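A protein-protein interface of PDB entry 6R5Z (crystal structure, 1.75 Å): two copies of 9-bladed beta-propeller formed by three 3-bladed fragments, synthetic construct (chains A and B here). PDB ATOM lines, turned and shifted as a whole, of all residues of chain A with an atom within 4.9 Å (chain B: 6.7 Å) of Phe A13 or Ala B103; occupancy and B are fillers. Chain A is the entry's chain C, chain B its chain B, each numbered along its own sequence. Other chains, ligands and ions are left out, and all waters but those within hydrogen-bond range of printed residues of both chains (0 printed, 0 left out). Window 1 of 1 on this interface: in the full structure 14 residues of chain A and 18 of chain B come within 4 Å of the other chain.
OG of Ser B96 lies within hydrogen-bond range of OD1 of Asp B98 (2.7 Å). The backbone carbonyl oxygen (O) of Val B111 is in hydrogen-bond range of the backbone NH (N) of Leu B124, 2.8 Å away. The backbone carbonyl oxygen (O) of Gly B92 lies within hydrogen-bond range of the backbone NH (N) of Ala B105, at 2.9 Å. The backbone NH (N) of Ala B103 sits at hydrogen-bond distance from the backbone carbonyl oxygen (O) of Ala B94 (2.9 Å). The backbone carbonyl oxygen (O) of Thr A19 lies within hydrogen-bond range of the backbone NH (N) of Ser A14 (2.8 Å). N of Ser B96 sits at hydrogen-bond distance from O of Thr B101, 2.9 Å away.
Among the printed residues, pairs that only touch across the chains: Trp A9 with Gly B92 (3.5 Å), Trp A9 with Val B93 (3.4 Å), Trp A9 with Ala B94 (3.7 Å), Trp A9 with Ala B103 (3.9 Å), Val A11 with Val B111 (3.6 Å), Phe A13 with Phe B95 (3.8 Å), Phe A13 with Ser B96 (3.5 Å), Phe A13 with Pro B97 (3.4 Å), Phe A13 with Thr B101 (3.5 Å), Phe A13 with Ala B103 (3.98 Å), Ser A14 with Pro B97 (3.5 Å), Pro A15 with Pro B97 (3.3 Å) and Ile A20 with Leu B113 (3.8 Å).
Ala A12 touches none of the printed residues of chain B. Printed residues of chain B within 4 Å of Phe A13: Phe B95 (3.8 Å), Ser B96 (3.5 Å), Pro B97 (3.4 Å), Thr B101 (3.5 Å) and Ala B103 (3.98 Å). Of the printed residues of chain B, Pro A15 touches Pro B97. Of the printed residues of chain A, Gly B92 touches Trp A9. Printed residues of chain A within 4 Å of Ser B96: Phe A13. Printed residues of chain A within 4 Å of Thr B101: Phe A13 (3.5 Å). Printed residues of chain A within 4 Å of Ala B103: Trp A9 and Phe A13. The nearest printed residue of chain B that does not touch Phe A13 is Ala B94 (4.3 Å).
Of the 19 printed residues of chain B, 10 touch a printed residue of chain A. Hydrophobic or aromatic side chains of chain A that line the printed part of chain B: Trp A9, Val A11, Phe A13 and Ile A20. Among the printed residues, 13 pairs touch across the chains.
No position is printed for both chains.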
ATOM      1  N   TRP A   9       9.666  -6.321  -7.747  1.00  0.00           N
ATOM      2  CA  TRP A   9       9.578  -7.705  -7.219  1.00  0.00           C
ATOM      3  C   TRP A   9       8.516  -7.903  -6.147  1.00  0.00           C
ATOM      4  O   TRP A   9       7.660  -8.790  -6.266  1.00  0.00           O
ATOM      5  CB  TRP A   9      10.948  -8.223  -6.640  1.00  0.00           C
ATOM      6  CG  TRP A   9      11.705  -9.053  -7.587  1.00  0.00           C
ATOM      7  CD1 TRP A   9      12.769  -8.667  -8.377  1.00  0.00           C
ATOM      8  CD2 TRP A   9      11.440 -10.412  -7.909  1.00  0.00           C
ATOM      9  NE1 TRP A   9      13.190  -9.723  -9.151  1.00  0.00           N
ATOM     10  CE2 TRP A   9      12.386 -10.803  -8.888  1.00  0.00           C
ATOM     11  CE3 TRP A   9      10.498 -11.345  -7.463  1.00  0.00           C
ATOM     12  CZ2 TRP A   9      12.410 -12.093  -9.422  1.00  0.00           C
ATOM     13  CZ3 TRP A   9      10.533 -12.619  -7.978  1.00  0.00           C
ATOM     14  CH2 TRP A   9      11.476 -12.984  -8.957  1.00  0.00           C
ATOM     15  N   VAL A  11       9.307  -9.256  -3.265  1.00  0.00           N
ATOM     16  CA  VAL A  11       9.689 -10.471  -2.528  1.00  0.00           C
ATOM     17  C   VAL A  11      11.135 -10.301  -2.179  1.00  0.00           C
ATOM     18  O   VAL A  11      11.891  -9.814  -3.024  1.00  0.00           O
ATOM     19  CB  VAL A  11       9.555 -11.718  -3.425  1.00  0.00           C
ATOM     20  CG1 VAL A  11      10.022 -12.967  -2.688  1.00  0.00           C
ATOM     21  CG2 VAL A  11       8.110 -11.847  -3.853  1.00  0.00           C
ATOM     22  N   ALA A  12      11.519 -10.776  -1.012  1.00  0.00           N
ATOM     23  CA  ALA A  12      12.956 -10.791  -0.677  1.00  0.00           C
ATOM     24  C   ALA A  12      13.232 -12.024   0.140  1.00  0.00           C
ATOM     25  O   ALA A  12      12.400 -12.472   0.972  1.00  0.00           O
ATOM     26  CB  ALA A  12      13.348  -9.587   0.120  1.00  0.00           C
ATOM     27  N   PHE A  13      14.386 -12.581  -0.079  1.00  0.00           N
ATOM     28  CA  PHE A  13      14.833 -13.732   0.770  1.00  0.00           C
ATOM     29  C   PHE A  13      15.738 -13.275   1.891  1.00  0.00           C
ATOM     30  O   PHE A  13      16.560 -12.391   1.662  1.00  0.00           O
ATOM     31  CB  PHE A  13      15.643 -14.696  -0.069  1.00  0.00           C
ATOM     32  CG  PHE A  13      14.868 -15.410  -1.087  1.00  0.00           C
ATOM     33  CD1 PHE A  13      14.104 -16.500  -0.740  1.00  0.00           C
ATOM     34  CD2 PHE A  13      14.826 -14.937  -2.415  1.00  0.00           C
ATOM     35  CE1 PHE A  13      13.349 -17.140  -1.711  1.00  0.00           C
ATOM     36  CE2 PHE A  13      14.106 -15.620  -3.386  1.00  0.00           C
ATOM     37  CZ  PHE A  13      13.354 -16.689  -3.015  1.00  0.00           C
ATOM     38  N   SER A  14      15.653 -13.895   3.076  1.00  0.00           N
ATOM     39  CA  SER A  14      16.641 -13.675   4.104  1.00  0.00           C
ATOM     40  C   SER A  14      18.002 -14.233   3.616  1.00  0.00           C
ATOM     41  O   SER A  14      18.045 -15.099   2.758  1.00  0.00           O
ATOM     42  CB  SER A  14      16.255 -14.333   5.415  1.00  0.00           C
ATOM     43  OG  SER A  14      16.267 -15.761   5.268  1.00  0.00           O
ATOM     44  N   PRO A  15      19.120 -13.618   4.022  1.00  0.00           N
ATOM     45  CA  PRO A  15      20.419 -14.123   3.536  1.00  0.00           C
ATOM     46  C   PRO A  15      20.643 -15.605   3.699  1.00  0.00           C
ATOM     47  O   PRO A  15      21.360 -16.224   2.900  1.00  0.00           O
ATOM     48  CB  PRO A  15      21.433 -13.317   4.356  1.00  0.00           C
ATOM     49  CG  PRO A  15      20.773 -12.051   4.599  1.00  0.00           C
ATOM     50  CD  PRO A  15      19.273 -12.347   4.737  1.00  0.00           C
ATOM     51  N   THR A  19      13.807 -17.589   5.515  1.00  0.00           N
ATOM     52  CA  THR A  19      12.620 -16.735   5.630  1.00  0.00           C
ATOM     53  C   THR A  19      12.469 -16.001   4.330  1.00  0.00           C
ATOM     54  O   THR A  19      13.443 -15.578   3.708  1.00  0.00           O
ATOM     55  CB  THR A  19      12.684 -15.690   6.791  1.00  0.00           C
ATOM     56  OG1 THR A  19      13.087 -16.321   8.001  1.00  0.00           O
ATOM     57  CG2 THR A  19      11.347 -15.035   7.009  1.00  0.00           C
ATOM     58  N   ILE A  20      11.210 -15.845   3.886  1.00  0.00           N
ATOM     59  CA  ILE A  20      10.892 -15.105   2.655  1.00  0.00           C
ATOM     60  C   ILE A  20       9.874 -14.034   3.034  1.00  0.00           C
ATOM     61  O   ILE A  20       8.963 -14.310   3.809  1.00  0.00           O
ATOM     62  CB  ILE A  20      10.263 -16.012   1.578  1.00  0.00           C
ATOM     63  CG1 ILE A  20      11.225 -17.190   1.242  1.00  0.00           C
ATOM     64  CG2 ILE A  20       9.952 -15.211   0.361  1.00  0.00           C
ATOM     65  CD1 ILE A  20      10.779 -18.547   1.674  1.00  0.00           C
ATOM     66  N   PHE A  54      15.605  -7.524   3.163  1.00  0.00           N
ATOM     67  CA  PHE A  54      16.177  -7.932   4.433  1.00  0.00           C
ATOM     68  C   PHE A  54      17.514  -7.327   4.659  1.00  0.00           C
ATOM     69  O   PHE A  54      18.301  -7.164   3.695  1.00  0.00           O
ATOM     70  CB  PHE A  54      16.487  -9.454   4.503  1.00  0.00           C
ATOM     71  CG  PHE A  54      15.345 -10.288   4.896  1.00  0.00           C
ATOM     72  CD1 PHE A  54      14.448 -10.683   3.938  1.00  0.00           C
ATOM     73  CD2 PHE A  54      15.181 -10.717   6.213  1.00  0.00           C
ATOM     74  CE1 PHE A  54      13.396 -11.487   4.262  1.00  0.00           C
ATOM     75  CE2 PHE A  54      14.076 -11.497   6.548  1.00  0.00           C
ATOM     76  CZ  PHE A  54      13.192 -11.888   5.559  1.00  0.00           C
ATOM     77  N   VAL B  70       7.533 -21.329 -15.831  1.00  0.00           N
ATOM     78  CA  VAL B  70       8.940 -21.221 -15.554  1.00  0.00           C
ATOM     79  C   VAL B  70       9.551 -22.580 -15.925  1.00  0.00           C
ATOM     80  O   VAL B  70       8.963 -23.599 -15.639  1.00  0.00           O
ATOM     81  CB  VAL B  70       9.223 -20.959 -14.052  1.00  0.00           C
ATOM     82  CG1 VAL B  70      10.712 -21.204 -13.662  1.00  0.00           C
ATOM     83  CG2 VAL B  70       8.845 -19.553 -13.702  1.00  0.00           C
ATOM     84  N   HIS B  86       0.967 -20.480 -12.843  1.00  0.00           N
ATOM     85  CA  HIS B  86       0.633 -19.083 -13.070  1.00  0.00           C
ATOM     86  C   HIS B  86      -0.464 -18.975 -14.148  1.00  0.00           C
ATOM     87  O   HIS B  86      -0.489 -19.735 -15.122  1.00  0.00           O
ATOM     88  CB  HIS B  86       1.845 -18.261 -13.478  1.00  0.00           C
ATOM     89  CG  HIS B  86       2.755 -17.924 -12.338  1.00  0.00           C
ATOM     90  ND1 HIS B  86       2.475 -16.916 -11.439  1.00  0.00           N
ATOM     91  CD2 HIS B  86       3.953 -18.446 -11.968  1.00  0.00           C
ATOM     92  CE1 HIS B  86       3.469 -16.852 -10.558  1.00  0.00           C
ATOM     93  NE2 HIS B  86       4.357 -17.777 -10.854  1.00  0.00           N
ATOM     94  N   GLY B  92       9.346 -12.661 -13.835  1.00  0.00           N
ATOM     95  CA  GLY B  92      10.460 -12.732 -12.902  1.00  0.00           C
ATOM     96  C   GLY B  92      10.611 -14.050 -12.215  1.00  0.00           C
ATOM     97  O   GLY B  92       9.643 -14.750 -11.918  1.00  0.00           O
ATOM     98  N   VAL B  93      11.872 -14.441 -12.044  1.00  0.00           N
ATOM     99  CA  VAL B  93      12.154 -15.661 -11.366  1.00  0.00           C
ATOM    100  C   VAL B  93      13.455 -15.461 -10.592  1.00  0.00           C
ATOM    101  O   VAL B  93      14.367 -14.733 -11.057  1.00  0.00           O
ATOM    102  CB  VAL B  93      12.197 -16.871 -12.351  1.00  0.00           C
ATOM    103  CG1 VAL B  93      13.311 -16.728 -13.400  1.00  0.00           C
ATOM    104  CG2 VAL B  93      12.293 -18.180 -11.572  1.00  0.00           C
ATOM    105  N   ALA B  94      13.514 -16.005  -9.366  1.00  0.00           N
ATOM    106  CA  ALA B  94      14.743 -15.910  -8.563  1.00  0.00           C
ATOM    107  C   ALA B  94      14.890 -17.088  -7.642  1.00  0.00           C
ATOM    108  O   ALA B  94      13.905 -17.631  -7.133  1.00  0.00           O
ATOM    109  CB  ALA B  94      14.759 -14.693  -7.697  1.00  0.00           C
ATOM    110  N   PHE B  95      16.115 -17.505  -7.455  1.00  0.00           N
ATOM    111  CA  PHE B  95      16.389 -18.555  -6.462  1.00  0.00           C
ATOM    112  C   PHE B  95      16.651 -17.938  -5.114  1.00  0.00           C
ATOM    113  O   PHE B  95      17.310 -16.893  -5.040  1.00  0.00           O
ATOM    114  CB  PHE B  95      17.644 -19.370  -6.865  1.00  0.00           C
ATOM    115  CG  PHE B  95      17.439 -20.278  -8.062  1.00  0.00           C
ATOM    116  CD1 PHE B  95      17.564 -19.774  -9.365  1.00  0.00           C
ATOM    117  CD2 PHE B  95      17.083 -21.613  -7.904  1.00  0.00           C
ATOM    118  CE1 PHE B  95      17.410 -20.597 -10.488  1.00  0.00           C
ATOM    119  CE2 PHE B  95      16.954 -22.468  -9.027  1.00  0.00           C
ATOM    120  CZ  PHE B  95      17.064 -21.936 -10.314  1.00  0.00           C
ATOM    121  N   SER B  96      16.334 -18.647  -4.037  1.00  0.00           N
ATOM    122  CA  SER B  96      16.816 -18.261  -2.728  1.00  0.00           C
ATOM    123  C   SER B  96      18.349 -18.394  -2.613  1.00  0.00           C
ATOM    124  O   SER B  96      18.923 -19.147  -3.366  1.00  0.00           O
ATOM    125  CB  SER B  96      16.188 -19.123  -1.628  1.00  0.00           C
ATOM    126  OG  SER B  96      16.515 -20.478  -1.819  1.00  0.00           O
ATOM    127  N   PRO B  97      18.966 -17.700  -1.647  1.00  0.00           N
ATOM    128  CA  PRO B  97      20.430 -17.721  -1.521  1.00  0.00           C
ATOM    129  C   PRO B  97      20.933 -19.097  -1.187  1.00  0.00           C
ATOM    130  O   PRO B  97      22.105 -19.363  -1.469  1.00  0.00           O
ATOM    131  CB  PRO B  97      20.723 -16.749  -0.329  1.00  0.00           C
ATOM    132  CG  PRO B  97      19.525 -15.855  -0.317  1.00  0.00           C
ATOM    133  CD  PRO B  97      18.360 -16.597  -0.891  1.00  0.00           C
ATOM    134  N   ASP B  98      20.110 -19.950  -0.582  1.00  0.00           N
ATOM    135  CA  ASP B  98      20.576 -21.339  -0.253  1.00  0.00           C
ATOM    136  C   ASP B  98      20.178 -22.299  -1.352  1.00  0.00           C
ATOM    137  O   ASP B  98      20.486 -23.465  -1.279  1.00  0.00           O
ATOM    138  CB  ASP B  98      20.055 -21.816   1.096  1.00  0.00           C
ATOM    139  CG  ASP B  98      18.574 -22.123   1.128  1.00  0.00           C
ATOM    140  OD1 ASP B  98      17.787 -21.751   0.240  1.00  0.00           O
ATOM    141  OD2 ASP B  98      18.216 -22.751   2.168  1.00  0.00           O
ATOM    142  N   THR B 101      14.700 -22.868  -2.609  1.00  0.00           N
ATOM    143  CA  THR B 101      13.405 -22.419  -3.067  1.00  0.00           C
ATOM    144  C   THR B 101      13.567 -21.467  -4.225  1.00  0.00           C
ATOM    145  O   THR B 101      14.617 -20.914  -4.466  1.00  0.00           O
ATOM    146  CB  THR B 101      12.561 -21.782  -1.958  1.00  0.00           C
ATOM    147  OG1 THR B 101      13.201 -20.642  -1.424  1.00  0.00           O
ATOM    148  CG2 THR B 101      12.291 -22.734  -0.861  1.00  0.00           C
ATOM    149  N   ILE B 102      12.465 -21.304  -4.965  1.00  0.00           N
ATOM    150  CA  ILE B 102      12.410 -20.489  -6.170  1.00  0.00           C
ATOM    151  C   ILE B 102      11.123 -19.649  -6.060  1.00  0.00           C
ATOM    152  O   ILE B 102      10.096 -20.168  -5.692  1.00  0.00           O
ATOM    153  CB  ILE B 102      12.294 -21.360  -7.470  1.00  0.00           C
ATOM    154  CG1 ILE B 102      13.511 -22.261  -7.667  1.00  0.00           C
ATOM    155  CG2 ILE B 102      12.121 -20.472  -8.717  1.00  0.00           C
ATOM    156  CD1 ILE B 102      13.289 -23.476  -8.547  1.00  0.00           C
ATOM    157  N   ALA B 103      11.221 -18.348  -6.292  1.00  0.00           N
ATOM    158  CA  ALA B 103      10.060 -17.454  -6.364  1.00  0.00           C
ATOM    159  C   ALA B 103       9.843 -17.039  -7.821  1.00  0.00           C
ATOM    160  O   ALA B 103      10.810 -16.758  -8.562  1.00  0.00           O
ATOM    161  CB  ALA B 103      10.295 -16.203  -5.521  1.00  0.00           C
ATOM    162  N   SER B 104       8.586 -16.964  -8.211  1.00  0.00           N
ATOM    163  CA  SER B 104       8.241 -16.607  -9.533  1.00  0.00           C
ATOM    164  C   SER B 104       7.134 -15.559  -9.436  1.00  0.00           C
ATOM    165  O   SER B 104       6.335 -15.597  -8.524  1.00  0.00           O
ATOM    166  CB  SER B 104       7.826 -17.806 -10.380  1.00  0.00           C
ATOM    167  OG  SER B 104       6.689 -18.465  -9.822  1.00  0.00           O
ATOM    168  N   ALA B 105       7.156 -14.622 -10.372  1.00  0.00           N
ATOM    169  CA  ALA B 105       6.229 -13.481 -10.369  1.00  0.00           C
ATOM    170  C   ALA B 105       5.625 -13.278 -11.708  1.00  0.00           C
ATOM    171  O   ALA B 105       6.339 -13.158 -12.711  1.00  0.00           O
ATOM    172  CB  ALA B 105       6.996 -12.218  -9.963  1.00  0.00           C
ATOM    173  N   VAL B 111       2.668 -14.122  -6.922  1.00  0.00           N
ATOM    174  CA  VAL B 111       3.980 -14.658  -6.639  1.00  0.00           C
ATOM    175  C   VAL B 111       3.799 -16.059  -6.091  1.00  0.00           C
ATOM    176  O   VAL B 111       3.000 -16.265  -5.180  1.00  0.00           O
ATOM    177  CB  VAL B 111       4.709 -13.810  -5.589  1.00  0.00           C
ATOM    178  CG1 VAL B 111       6.026 -14.480  -5.224  1.00  0.00           C
ATOM    179  CG2 VAL B 111       4.915 -12.381  -6.096  1.00  0.00           C
ATOM    180  N   LYS B 112       4.525 -17.006  -6.668  1.00  0.00           N
ATOM    181  CA  LYS B 112       4.512 -18.381  -6.201  1.00  0.00           C
ATOM    182  C   LYS B 112       5.921 -18.745  -5.703  1.00  0.00           C
ATOM    183  O   LYS B 112       6.953 -18.258  -6.182  1.00  0.00           O
ATOM    184  CB  LYS B 112       4.039 -19.308  -7.300  1.00  0.00           C
ATOM    185  CG  LYS B 112       2.563 -19.051  -7.614  1.00  0.00           C
ATOM    186  CD  LYS B 112       2.070 -19.900  -8.751  1.00  0.00           C
ATOM    187  CE  LYS B 112       0.637 -19.568  -9.057  1.00  0.00           C
ATOM    188  NZ  LYS B 112      -0.348 -20.149  -8.085  1.00  0.00           N
ATOM    189  N   LEU B 113       5.916 -19.622  -4.698  1.00  0.00           N
ATOM    190  CA  LEU B 113       7.118 -20.181  -4.133  1.00  0.00           C
ATOM    191  C   LEU B 113       7.137 -21.688  -4.363  1.00  0.00           C
ATOM    192  O   LEU B 113       6.137 -22.375  -4.119  1.00  0.00           O
ATOM    193  CB  LEU B 113       7.140 -19.915  -2.657  1.00  0.00           C
ATOM    194  CG  LEU B 113       8.421 -20.311  -1.903  1.00  0.00           C
ATOM    195  CD1 LEU B 113       9.522 -19.348  -2.221  1.00  0.00           C
ATOM    196  CD2 LEU B 113       8.096 -20.330  -0.403  1.00  0.00           C
ATOM    197  N   TRP B 114       8.258 -22.185  -4.887  1.00  0.00           N
ATOM    198  CA  TRP B 114       8.417 -23.570  -5.264  1.00  0.00           C
ATOM    199  C   TRP B 114       9.649 -24.105  -4.581  1.00  0.00           C
ATOM    200  O   TRP B 114      10.604 -23.370  -4.335  1.00  0.00           O
ATOM    201  CB  TRP B 114       8.654 -23.723  -6.779  1.00  0.00           C
ATOM    202  CG  TRP B 114       7.730 -22.863  -7.652  1.00  0.00           C
ATOM    203  CD1 TRP B 114       7.866 -21.533  -7.891  1.00  0.00           C
ATOM    204  CD2 TRP B 114       6.601 -23.297  -8.433  1.00  0.00           C
ATOM    205  NE1 TRP B 114       6.859 -21.082  -8.711  1.00  0.00           N
ATOM    206  CE2 TRP B 114       6.093 -22.140  -9.102  1.00  0.00           C
ATOM    207  CE3 TRP B 114       6.019 -24.514  -8.684  1.00  0.00           C
ATOM    208  CZ2 TRP B 114       4.985 -22.177  -9.930  1.00  0.00           C
ATOM    209  CZ3 TRP B 114       4.852 -24.544  -9.473  1.00  0.00           C
ATOM    210  CH2 TRP B 114       4.374 -23.378 -10.115  1.00  0.00           C
ATOM    211  N   LEU B 124       2.195 -16.771  -2.510  1.00  0.00           N
ATOM    212  CA  LEU B 124       2.461 -15.739  -1.490  1.00  0.00           C
ATOM    213  C   LEU B 124       1.500 -14.580  -1.641  1.00  0.00           C
ATOM    214  O   LEU B 124       1.114 -13.967  -0.669  1.00  0.00           O
ATOM    215  CB  LEU B 124       3.883 -15.228  -1.611  1.00  0.00           C
ATOM    216  CG  LEU B 124       4.966 -16.306  -1.572  1.00  0.00           C
ATOM    217  CD1 LEU B 124       6.347 -15.698  -1.522  1.00  0.00           C
ATOM    218  CD2 LEU B 124       4.751 -17.241  -0.388  1.00  0.00           C
